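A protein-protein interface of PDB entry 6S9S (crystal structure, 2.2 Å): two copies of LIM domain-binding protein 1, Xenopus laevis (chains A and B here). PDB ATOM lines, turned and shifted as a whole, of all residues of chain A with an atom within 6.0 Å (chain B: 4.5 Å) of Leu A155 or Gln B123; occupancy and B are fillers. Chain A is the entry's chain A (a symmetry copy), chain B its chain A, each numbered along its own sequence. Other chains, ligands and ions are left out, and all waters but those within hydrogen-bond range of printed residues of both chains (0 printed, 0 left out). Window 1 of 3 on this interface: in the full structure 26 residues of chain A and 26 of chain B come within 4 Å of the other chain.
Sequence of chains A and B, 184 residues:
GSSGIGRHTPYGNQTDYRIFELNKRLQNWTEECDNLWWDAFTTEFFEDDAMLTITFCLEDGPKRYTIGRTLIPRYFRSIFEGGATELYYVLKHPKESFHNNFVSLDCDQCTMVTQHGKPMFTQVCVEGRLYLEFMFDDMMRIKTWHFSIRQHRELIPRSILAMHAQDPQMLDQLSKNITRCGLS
Leu A155 touches its own counterpart, Leu B155.
Leu A155 touches Ile B156, and with the chains exchanged Ile A156 touches Leu B155.
Leu A155 touches Pro B157, and with the chains exchanged Pro A157 touches Leu B155.
Ile B156 touches its own counterpart, Ile A156.
Positions printed for both chains: 115, 120, 122, 123, 124, 125, 153, 154, 155, 156 and 157.
The side-chain amide oxygen of Gln B123 sits at hydrogen-bond distance from the side-chain amide nitrogen of Gln A123 (3.1 Å).
N of Ile B156 is in hydrogen-bond range of O of Ile A156, 3.2 Å away.
Among the printed residues, pairs that only touch across the chains: Gln A123 with Leu B155 (3.9 Å), Glu A154 with Pro B157 (3.5 Å), Leu A155 with Gln B123 (3.9 Å), Leu A155 with Leu B155 (3.5 Å), Leu A155 with Ile B156 (3.3 Å), Leu A155 with Pro B157 (3.7 Å), Ile A156 with Leu B155 (3.3 Å), Pro A157 with Glu B154 (3.5 Å) and Pro A157 with Leu B155 (3.7 Å).
OE1 of Gln B123 sits at hydrogen-bond distance from NE2 of Gln B115 (3.4 Å).
The side-chain sulfur of Cys B125 sits at hydrogen-bond distance from the side-chain amide nitrogen of Gln B123 (3.3 Å).
N of Gln B123 is in hydrogen-bond range of O of Leu B155, 2.9 Å away.
The side-chain amide nitrogen of Gln A115 sits at hydrogen-bond distance from the side-chain amide oxygen of Gln A123 (3.4 Å).
The side-chain amide nitrogen of Gln A123 lies within hydrogen-bond range of the side-chain sulfur of Cys A125, 3.4 Å away.
N of Gln A123 is in hydrogen-bond range of O of Leu A155 (2.9 Å).
Printed residues of chain B within 4 Å of Gln A123: Gln B123 (3.1 Å) and Leu B155 (3.9 Å).
Printed residues of chain B within 4 Å of Glu A154: Pro B157 (3.5 Å).
Printed residues of chain B within 4 Å of Pro A157: Glu B154 (3.5 Å) and Leu B155 (3.7 Å).
Val B113 touches none of the printed residues of chain A.
Gln B123 touches just these residues of chain A: Gln A123 and Leu A155.
Val B124 touches none of the printed residues of chain A.
Printed residues of chain A within 4 Å of Glu B154: Pro A157.
Of the printed residues of chain A, Leu B155 touches Gln A123, Leu A155, Ile A156 and Pro A157.
Hydrophobic or aromatic side chains of chain A within 4 Å of the printed part of chain B: Leu A155 and Ile A156.
Of the 13 printed residues of chain B, 5 touch a printed residue of chain A.
Hydrophobic or aromatic side chains of chain B within 4 Å of the printed part of chain A: Leu B155 and Ile B156.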
ATOM      1  N   TYR A  88      22.309 -11.462 -12.520  1.00  0.00           N
ATOM      2  CA  TYR A  88      21.655 -10.455 -11.644  1.00  0.00           C
ATOM      3  C   TYR A  88      20.207 -10.237 -12.065  1.00  0.00           C
ATOM      4  O   TYR A  88      19.838 -10.523 -13.220  1.00  0.00           O
ATOM      5  CB  TYR A  88      22.445  -9.154 -11.586  1.00  0.00           C
ATOM      6  CG  TYR A  88      22.796  -8.571 -12.928  1.00  0.00           C
ATOM      7  CD1 TYR A  88      21.887  -7.791 -13.628  1.00  0.00           C
ATOM      8  CD2 TYR A  88      24.058  -8.746 -13.470  1.00  0.00           C
ATOM      9  CE1 TYR A  88      22.209  -7.250 -14.863  1.00  0.00           C
ATOM     10  CE2 TYR A  88      24.402  -8.189 -14.692  1.00  0.00           C
ATOM     11  CZ  TYR A  88      23.468  -7.464 -15.406  1.00  0.00           C
ATOM     12  OH  TYR A  88      23.797  -6.926 -16.618  1.00  0.00           O
ATOM     13  N   GLN A 115      24.818 -13.801 -18.406  1.00  0.00           N
ATOM     14  CA  GLN A 115      25.759 -13.635 -19.527  1.00  0.00           C
ATOM     15  C   GLN A 115      26.473 -14.972 -19.691  1.00  0.00           C
ATOM     16  O   GLN A 115      27.053 -15.387 -18.716  1.00  0.00           O
ATOM     17  CB  GLN A 115      26.696 -12.475 -19.207  1.00  0.00           C
ATOM     18  CG  GLN A 115      25.948 -11.169 -18.941  1.00  0.00           C
ATOM     19  CD  GLN A 115      26.877  -9.983 -18.823  1.00  0.00           C
ATOM     20  OE1 GLN A 115      28.104 -10.121 -18.752  1.00  0.00           O
ATOM     21  NE2 GLN A 115      26.284  -8.799 -18.798  1.00  0.00           N
ATOM     22  N   MET A 120      32.186 -13.526 -23.365  1.00  0.00           N
ATOM     23  CA  MET A 120      30.732 -13.290 -23.588  1.00  0.00           C
ATOM     24  C   MET A 120      30.411 -13.421 -25.081  1.00  0.00           C
ATOM     25  O   MET A 120      31.074 -12.760 -25.895  1.00  0.00           O
ATOM     26  CB  MET A 120      30.329 -11.899 -23.084  1.00  0.00           C
ATOM     27  CG  MET A 120      29.321 -11.169 -23.973  1.00  0.00           C
ATOM     28  SD  MET A 120      27.573 -11.507 -23.573  1.00  0.00           S
ATOM     29  CE  MET A 120      27.509 -10.682 -21.982  1.00  0.00           C
ATOM     30  N   PHE A 121      29.448 -14.278 -25.410  1.00  0.00           N
ATOM     31  CA  PHE A 121      28.961 -14.536 -26.786  1.00  0.00           C
ATOM     32  C   PHE A 121      27.427 -14.444 -26.797  1.00  0.00           C
ATOM     33  O   PHE A 121      26.857 -14.426 -27.908  1.00  0.00           O
ATOM     34  CB  PHE A 121      29.501 -15.884 -27.302  1.00  0.00           C
ATOM     35  CG  PHE A 121      28.867 -17.107 -26.690  1.00  0.00           C
ATOM     36  CD1 PHE A 121      27.710 -17.659 -27.221  1.00  0.00           C
ATOM     37  CD2 PHE A 121      29.431 -17.718 -25.575  1.00  0.00           C
ATOM     38  CE1 PHE A 121      27.123 -18.773 -26.626  1.00  0.00           C
ATOM     39  CE2 PHE A 121      28.862 -18.847 -24.998  1.00  0.00           C
ATOM     40  CZ  PHE A 121      27.700 -19.371 -25.517  1.00  0.00           C
ATOM     41  N   THR A 122      26.771 -14.391 -25.625  1.00  0.00           N
ATOM     42  CA  THR A 122      25.296 -14.194 -25.503  1.00  0.00           C
ATOM     43  C   THR A 122      24.896 -13.640 -24.130  1.00  0.00           C
ATOM     44  O   THR A 122      25.489 -14.067 -23.124  1.00  0.00           O
ATOM     45  CB  THR A 122      24.538 -15.503 -25.725  1.00  0.00           C
ATOM     46  OG1 THR A 122      24.752 -15.885 -27.079  1.00  0.00           O
ATOM     47  CG2 THR A 122      23.053 -15.361 -25.477  1.00  0.00           C
ATOM     48  N   GLN A 123      23.913 -12.733 -24.096  1.00  0.00           N
ATOM     49  CA  GLN A 123      23.222 -12.282 -22.859  1.00  0.00           C
ATOM     50  C   GLN A 123      21.776 -12.770 -22.905  1.00  0.00           C
ATOM     51  O   GLN A 123      21.171 -12.707 -23.959  1.00  0.00           O
ATOM     52  CB  GLN A 123      23.283 -10.766 -22.707  1.00  0.00           C
ATOM     53  CG  GLN A 123      22.603 -10.306 -21.428  1.00  0.00           C
ATOM     54  CD  GLN A 123      22.648  -8.820 -21.199  1.00  0.00           C
ATOM     55  OE1 GLN A 123      23.693  -8.218 -20.968  1.00  0.00           O
ATOM     56  NE2 GLN A 123      21.480  -8.227 -21.285  1.00  0.00           N
ATOM     57  N   VAL A 124      21.263 -13.299 -21.805  1.00  0.00           N
ATOM     58  CA  VAL A 124      19.875 -13.852 -21.744  1.00  0.00           C
ATOM     59  C   VAL A 124      19.110 -13.003 -20.738  1.00  0.00           C
ATOM     60  O   VAL A 124      19.593 -12.853 -19.589  1.00  0.00           O
ATOM     61  CB  VAL A 124      19.832 -15.341 -21.349  1.00  0.00           C
ATOM     62  CG1 VAL A 124      18.415 -15.867 -21.221  1.00  0.00           C
ATOM     63  CG2 VAL A 124      20.631 -16.208 -22.312  1.00  0.00           C
ATOM     64  N   CYS A 125      17.988 -12.441 -21.187  1.00  0.00           N
ATOM     65  CA  CYS A 125      17.070 -11.643 -20.357  1.00  0.00           C
ATOM     66  C   CYS A 125      15.790 -12.448 -20.264  1.00  0.00           C
ATOM     67  O   CYS A 125      15.225 -12.765 -21.306  1.00  0.00           O
ATOM     68  CB  CYS A 125      16.826 -10.277 -20.977  1.00  0.00           C
ATOM     69  SG  CYS A 125      18.348  -9.407 -21.430  1.00  0.00           S
ATOM     70  N   ARG A 153      14.496 -13.050 -24.207  1.00  0.00           N
ATOM     71  CA  ARG A 153      15.154 -12.679 -25.480  1.00  0.00           C
ATOM     72  C   ARG A 153      16.641 -12.901 -25.264  1.00  0.00           C
ATOM     73  O   ARG A 153      17.073 -12.845 -24.119  1.00  0.00           O
ATOM     74  CB  ARG A 153      14.801 -11.255 -25.945  1.00  0.00           C
ATOM     75  CG  ARG A 153      15.014 -10.164 -24.906  1.00  0.00           C
ATOM     76  CD  ARG A 153      14.924  -8.744 -25.473  1.00  0.00           C
ATOM     77  NE  ARG A 153      14.655  -7.788 -24.394  1.00  0.00           N
ATOM     78  CZ  ARG A 153      15.514  -7.429 -23.417  1.00  0.00           C
ATOM     79  NH1 ARG A 153      16.753  -7.900 -23.375  1.00  0.00           N
ATOM     80  NH2 ARG A 153      15.125  -6.585 -22.473  1.00  0.00           N
ATOM     81  N   GLU A 154      17.366 -13.184 -26.332  1.00  0.00           N
ATOM     82  CA  GLU A 154      18.830 -13.376 -26.283  1.00  0.00           C
ATOM     83  C   GLU A 154      19.461 -12.284 -27.124  1.00  0.00           C
ATOM     84  O   GLU A 154      18.981 -12.084 -28.214  1.00  0.00           O
ATOM     85  CB  GLU A 154      19.225 -14.776 -26.779  1.00  0.00           C
ATOM     86  CG  GLU A 154      18.681 -15.896 -25.899  1.00  0.00           C
ATOM     87  CD  GLU A 154      19.015 -17.324 -26.313  1.00  0.00           C
ATOM     88  OE1 GLU A 154      19.994 -17.528 -27.071  1.00  0.00           O
ATOM     89  OE2 GLU A 154      18.291 -18.232 -25.876  1.00  0.00           O
ATOM     90  N   LEU A 155      20.498 -11.629 -26.605  1.00  0.00           N
ATOM     91  CA  LEU A 155      21.310 -10.616 -27.329  1.00  0.00           C
ATOM     92  C   LEU A 155      22.690 -11.194 -27.618  1.00  0.00           C
ATOM     93  O   LEU A 155      23.229 -11.873 -26.730  1.00  0.00           O
ATOM     94  CB  LEU A 155      21.451  -9.376 -26.457  1.00  0.00           C
ATOM     95  CG  LEU A 155      20.197  -8.986 -25.695  1.00  0.00           C
ATOM     96  CD1 LEU A 155      20.423  -7.676 -24.962  1.00  0.00           C
ATOM     97  CD2 LEU A 155      19.019  -8.865 -26.636  1.00  0.00           C
ATOM     98  N   ILE A 156      23.254 -10.894 -28.789  1.00  0.00           N
ATOM     99  CA  ILE A 156      24.616 -11.365 -29.182  1.00  0.00           C
ATOM    100  C   ILE A 156      25.426 -10.137 -29.526  1.00  0.00           C
ATOM    101  O   ILE A 156      24.866  -9.183 -30.025  1.00  0.00           O
ATOM    102  CB  ILE A 156      24.555 -12.346 -30.368  1.00  0.00           C
ATOM    103  CG1 ILE A 156      23.791 -11.728 -31.542  1.00  0.00           C
ATOM    104  CG2 ILE A 156      23.927 -13.649 -29.930  1.00  0.00           C
ATOM    105  CD1 ILE A 156      24.020 -12.418 -32.867  1.00  0.00           C
ATOM    106  N   PRO A 157      26.759 -10.141 -29.342  1.00  0.00           N
ATOM    107  CA  PRO A 157      27.589  -9.027 -29.784  1.00  0.00           C
ATOM    108  C   PRO A 157      27.321  -8.760 -31.265  1.00  0.00           C
ATOM    109  O   PRO A 157      27.104  -9.716 -32.008  1.00  0.00           O
ATOM    110  CB  PRO A 157      29.026  -9.509 -29.553  1.00  0.00           C
ATOM    111  CG  PRO A 157      28.881 -10.528 -28.460  1.00  0.00           C
ATOM    112  CD  PRO A 157      27.552 -11.205 -28.732  1.00  0.00           C
ATOM    113  N   VAL B 113      25.364   0.569 -18.670  1.00  0.00           N
ATOM    114  CA  VAL B 113      24.435  -0.152 -19.577  1.00  0.00           C
ATOM    115  C   VAL B 113      23.325   0.833 -19.994  1.00  0.00           C
ATOM    116  O   VAL B 113      22.643   1.416 -19.114  1.00  0.00           O
ATOM    117  CB  VAL B 113      23.853  -1.425 -18.922  1.00  0.00           C
ATOM    118  CG1 VAL B 113      22.998  -2.243 -19.883  1.00  0.00           C
ATOM    119  CG2 VAL B 113      24.952  -2.307 -18.335  1.00  0.00           C
ATOM    120  N   THR B 114      23.141   1.002 -21.301  1.00  0.00           N
ATOM    121  CA  THR B 114      21.954   1.693 -21.859  1.00  0.00           C
ATOM    122  C   THR B 114      21.256   0.747 -22.828  1.00  0.00           C
ATOM    123  O   THR B 114      21.928  -0.105 -23.453  1.00  0.00           O
ATOM    124  CB  THR B 114      22.334   3.005 -22.537  1.00  0.00           C
ATOM    125  OG1 THR B 114      23.271   2.565 -23.501  1.00  0.00           O
ATOM    126  CG2 THR B 114      22.942   4.032 -21.614  1.00  0.00           C
ATOM    127  N   GLN B 115      19.942   0.875 -22.915  1.00  0.00           N
ATOM    128  CA  GLN B 115      19.126   0.111 -23.876  1.00  0.00           C
ATOM    129  C   GLN B 115      18.478   1.136 -24.801  1.00  0.00           C
ATOM    130  O   GLN B 115      17.806   1.985 -24.264  1.00  0.00           O
ATOM    131  CB  GLN B 115      18.123  -0.733 -23.097  1.00  0.00           C
ATOM    132  CG  GLN B 115      18.794  -1.677 -22.100  1.00  0.00           C
ATOM    133  CD  GLN B 115      17.820  -2.649 -21.477  1.00  0.00           C
ATOM    134  OE1 GLN B 115      16.598  -2.534 -21.627  1.00  0.00           O
ATOM    135  NE2 GLN B 115      18.369  -3.622 -20.763  1.00  0.00           N
ATOM    136  N   MET B 120      13.166  -2.217 -27.764  1.00  0.00           N
ATOM    137  CA  MET B 120      14.628  -2.488 -27.665  1.00  0.00           C
ATOM    138  C   MET B 120      15.117  -3.156 -28.954  1.00  0.00           C
ATOM    139  O   MET B 120      14.529  -4.168 -29.364  1.00  0.00           O
ATOM    140  CB  MET B 120      14.928  -3.388 -26.460  1.00  0.00           C
ATOM    141  CG  MET B 120      16.005  -4.445 -26.710  1.00  0.00           C
ATOM    142  SD  MET B 120      17.707  -3.891 -26.357  1.00  0.00           S
ATOM    143  CE  MET B 120      17.567  -3.747 -24.575  1.00  0.00           C
ATOM    144  N   THR B 122      18.825  -2.505 -29.519  1.00  0.00           N
ATOM    145  CA  THR B 122      20.270  -2.560 -29.148  1.00  0.00           C
ATOM    146  C   THR B 122      20.497  -2.291 -27.656  1.00  0.00           C
ATOM    147  O   THR B 122      19.809  -1.416 -27.101  1.00  0.00           O
ATOM    148  CB  THR B 122      21.090  -1.543 -29.943  1.00  0.00           C
ATOM    149  OG1 THR B 122      21.040  -1.942 -31.308  1.00  0.00           O
ATOM    150  CG2 THR B 122      22.532  -1.484 -29.493  1.00  0.00           C
ATOM    151  N   GLN B 123      21.440  -3.011 -27.037  1.00  0.00           N
ATOM    152  CA  GLN B 123      21.974  -2.717 -25.682  1.00  0.00           C
ATOM    153  C   GLN B 123      23.431  -2.281 -25.817  1.00  0.00           C
ATOM    154  O   GLN B 123      24.147  -2.872 -26.603  1.00  0.00           O
ATOM    155  CB  GLN B 123      21.847  -3.925 -24.759  1.00  0.00           C
ATOM    156  CG  GLN B 123      22.366  -3.616 -23.363  1.00  0.00           C
ATOM    157  CD  GLN B 123      22.249  -4.757 -22.390  1.00  0.00           C
ATOM    158  OE1 GLN B 123      21.165  -5.179 -21.994  1.00  0.00           O
ATOM    159  NE2 GLN B 123      23.399  -5.268 -22.018  1.00  0.00           N
ATOM    160  N   VAL B 124      23.835  -1.234 -25.114  1.00  0.00           N
ATOM    161  CA  VAL B 124      25.224  -0.689 -25.200  1.00  0.00           C
ATOM    162  C   VAL B 124      25.845  -0.852 -23.819  1.00  0.00           C
ATOM    163  O   VAL B 124      25.233  -0.387 -22.828  1.00  0.00           O
ATOM    164  CB  VAL B 124      25.271   0.785 -25.651  1.00  0.00           C
ATOM    165  CG1 VAL B 124      26.681   1.344 -25.663  1.00  0.00           C
ATOM    166  CG2 VAL B 124      24.612   0.985 -27.008  1.00  0.00           C
ATOM    167  N   CYS B 125      26.991  -1.530 -23.775  1.00  0.00           N
ATOM    168  CA  CYS B 125      27.785  -1.739 -22.553  1.00  0.00           C
ATOM    169  C   CYS B 125      29.072  -0.966 -22.757  1.00  0.00           C
ATOM    170  O   CYS B 125      29.760  -1.230 -23.738  1.00  0.00           O
ATOM    171  CB  CYS B 125      28.053  -3.218 -22.325  1.00  0.00           C
ATOM    172  SG  CYS B 125      26.563  -4.243 -22.415  1.00  0.00           S
ATOM    173  N   ARG B 153      30.816  -2.499 -26.249  1.00  0.00           N
ATOM    174  CA  ARG B 153      30.293  -3.508 -27.198  1.00  0.00           C
ATOM    175  C   ARG B 153      28.798  -3.253 -27.299  1.00  0.00           C
ATOM    176  O   ARG B 153      28.240  -2.709 -26.354  1.00  0.00           O
ATOM    177  CB  ARG B 153      30.649  -4.951 -26.796  1.00  0.00           C
ATOM    178  CG  ARG B 153      30.287  -5.333 -25.369  1.00  0.00           C
ATOM    179  CD  ARG B 153      30.394  -6.834 -25.085  1.00  0.00           C
ATOM    180  NE  ARG B 153      30.511  -7.066 -23.642  1.00  0.00           N
ATOM    181  CZ  ARG B 153      29.537  -6.881 -22.725  1.00  0.00           C
ATOM    182  NH1 ARG B 153      28.316  -6.500 -23.078  1.00  0.00           N
ATOM    183  NH2 ARG B 153      29.791  -7.086 -21.441  1.00  0.00           N
ATOM    184  N   GLU B 154      28.206  -3.602 -28.428  1.00  0.00           N
ATOM    185  CA  GLU B 154      26.753  -3.459 -28.652  1.00  0.00           C
ATOM    186  C   GLU B 154      26.185  -4.850 -28.852  1.00  0.00           C
ATOM    187  O   GLU B 154      26.777  -5.581 -29.609  1.00  0.00           O
ATOM    188  CB  GLU B 154      26.461  -2.546 -29.853  1.00  0.00           C
ATOM    189  CG  GLU B 154      26.939  -1.115 -29.644  1.00  0.00           C
ATOM    190  CD  GLU B 154      26.699  -0.132 -30.785  1.00  0.00           C
ATOM    191  OE1 GLU B 154      25.818  -0.391 -31.639  1.00  0.00           O
ATOM    192  OE2 GLU B 154      27.398   0.891 -30.817  1.00  0.00           O
ATOM    193  N   LEU B 155      25.077  -5.165 -28.184  1.00  0.00           N
ATOM    194  CA  LEU B 155      24.318  -6.432 -28.349  1.00  0.00           C
ATOM    195  C   LEU B 155      22.998  -6.139 -29.051  1.00  0.00           C
ATOM    196  O   LEU B 155      22.385  -5.111 -28.723  1.00  0.00           O
ATOM    197  CB  LEU B 155      24.041  -7.028 -26.974  1.00  0.00           C
ATOM    198  CG  LEU B 155      25.189  -6.916 -25.987  1.00  0.00           C
ATOM    199  CD1 LEU B 155      24.841  -7.647 -24.703  1.00  0.00           C
ATOM    200  CD2 LEU B 155      26.460  -7.477 -26.584  1.00  0.00           C
ATOM    201  N   ILE B 156      22.559  -7.031 -29.940  1.00  0.00           N
ATOM    202  CA  ILE B 156      21.264  -6.883 -30.672  1.00  0.00           C
ATOM    203  C   ILE B 156      20.459  -8.133 -30.402  1.00  0.00           C
ATOM    204  O   ILE B 156      21.041  -9.187 -30.255  1.00  0.00           O
ATOM    205  CB  ILE B 156      21.489  -6.676 -32.182  1.00  0.00           C
ATOM    206  CG1 ILE B 156      22.359  -7.797 -32.758  1.00  0.00           C
ATOM    207  CG2 ILE B 156      22.106  -5.319 -32.432  1.00  0.00           C
ATOM    208  CD1 ILE B 156      22.301  -7.919 -34.262  1.00  0.00           C
ATOM    209  N   PRO B 157      19.115  -8.074 -30.398  1.00  0.00           N
ATOM    210  CA  PRO B 157      18.304  -9.279 -30.273  1.00  0.00           C
ATOM    211  C   PRO B 157      18.727 -10.280 -31.349  1.00  0.00           C
ATOM    212  O   PRO B 157      19.055  -9.855 -32.455  1.00  0.00           O
ATOM    213  CB  PRO B 157      16.866  -8.795 -30.494  1.00  0.00           C
ATOM    214  CG  PRO B 157      16.922  -7.347 -30.097  1.00  0.00           C
ATOM    215  CD  PRO B 157      18.293  -6.874 -30.536  1.00  0.00           C
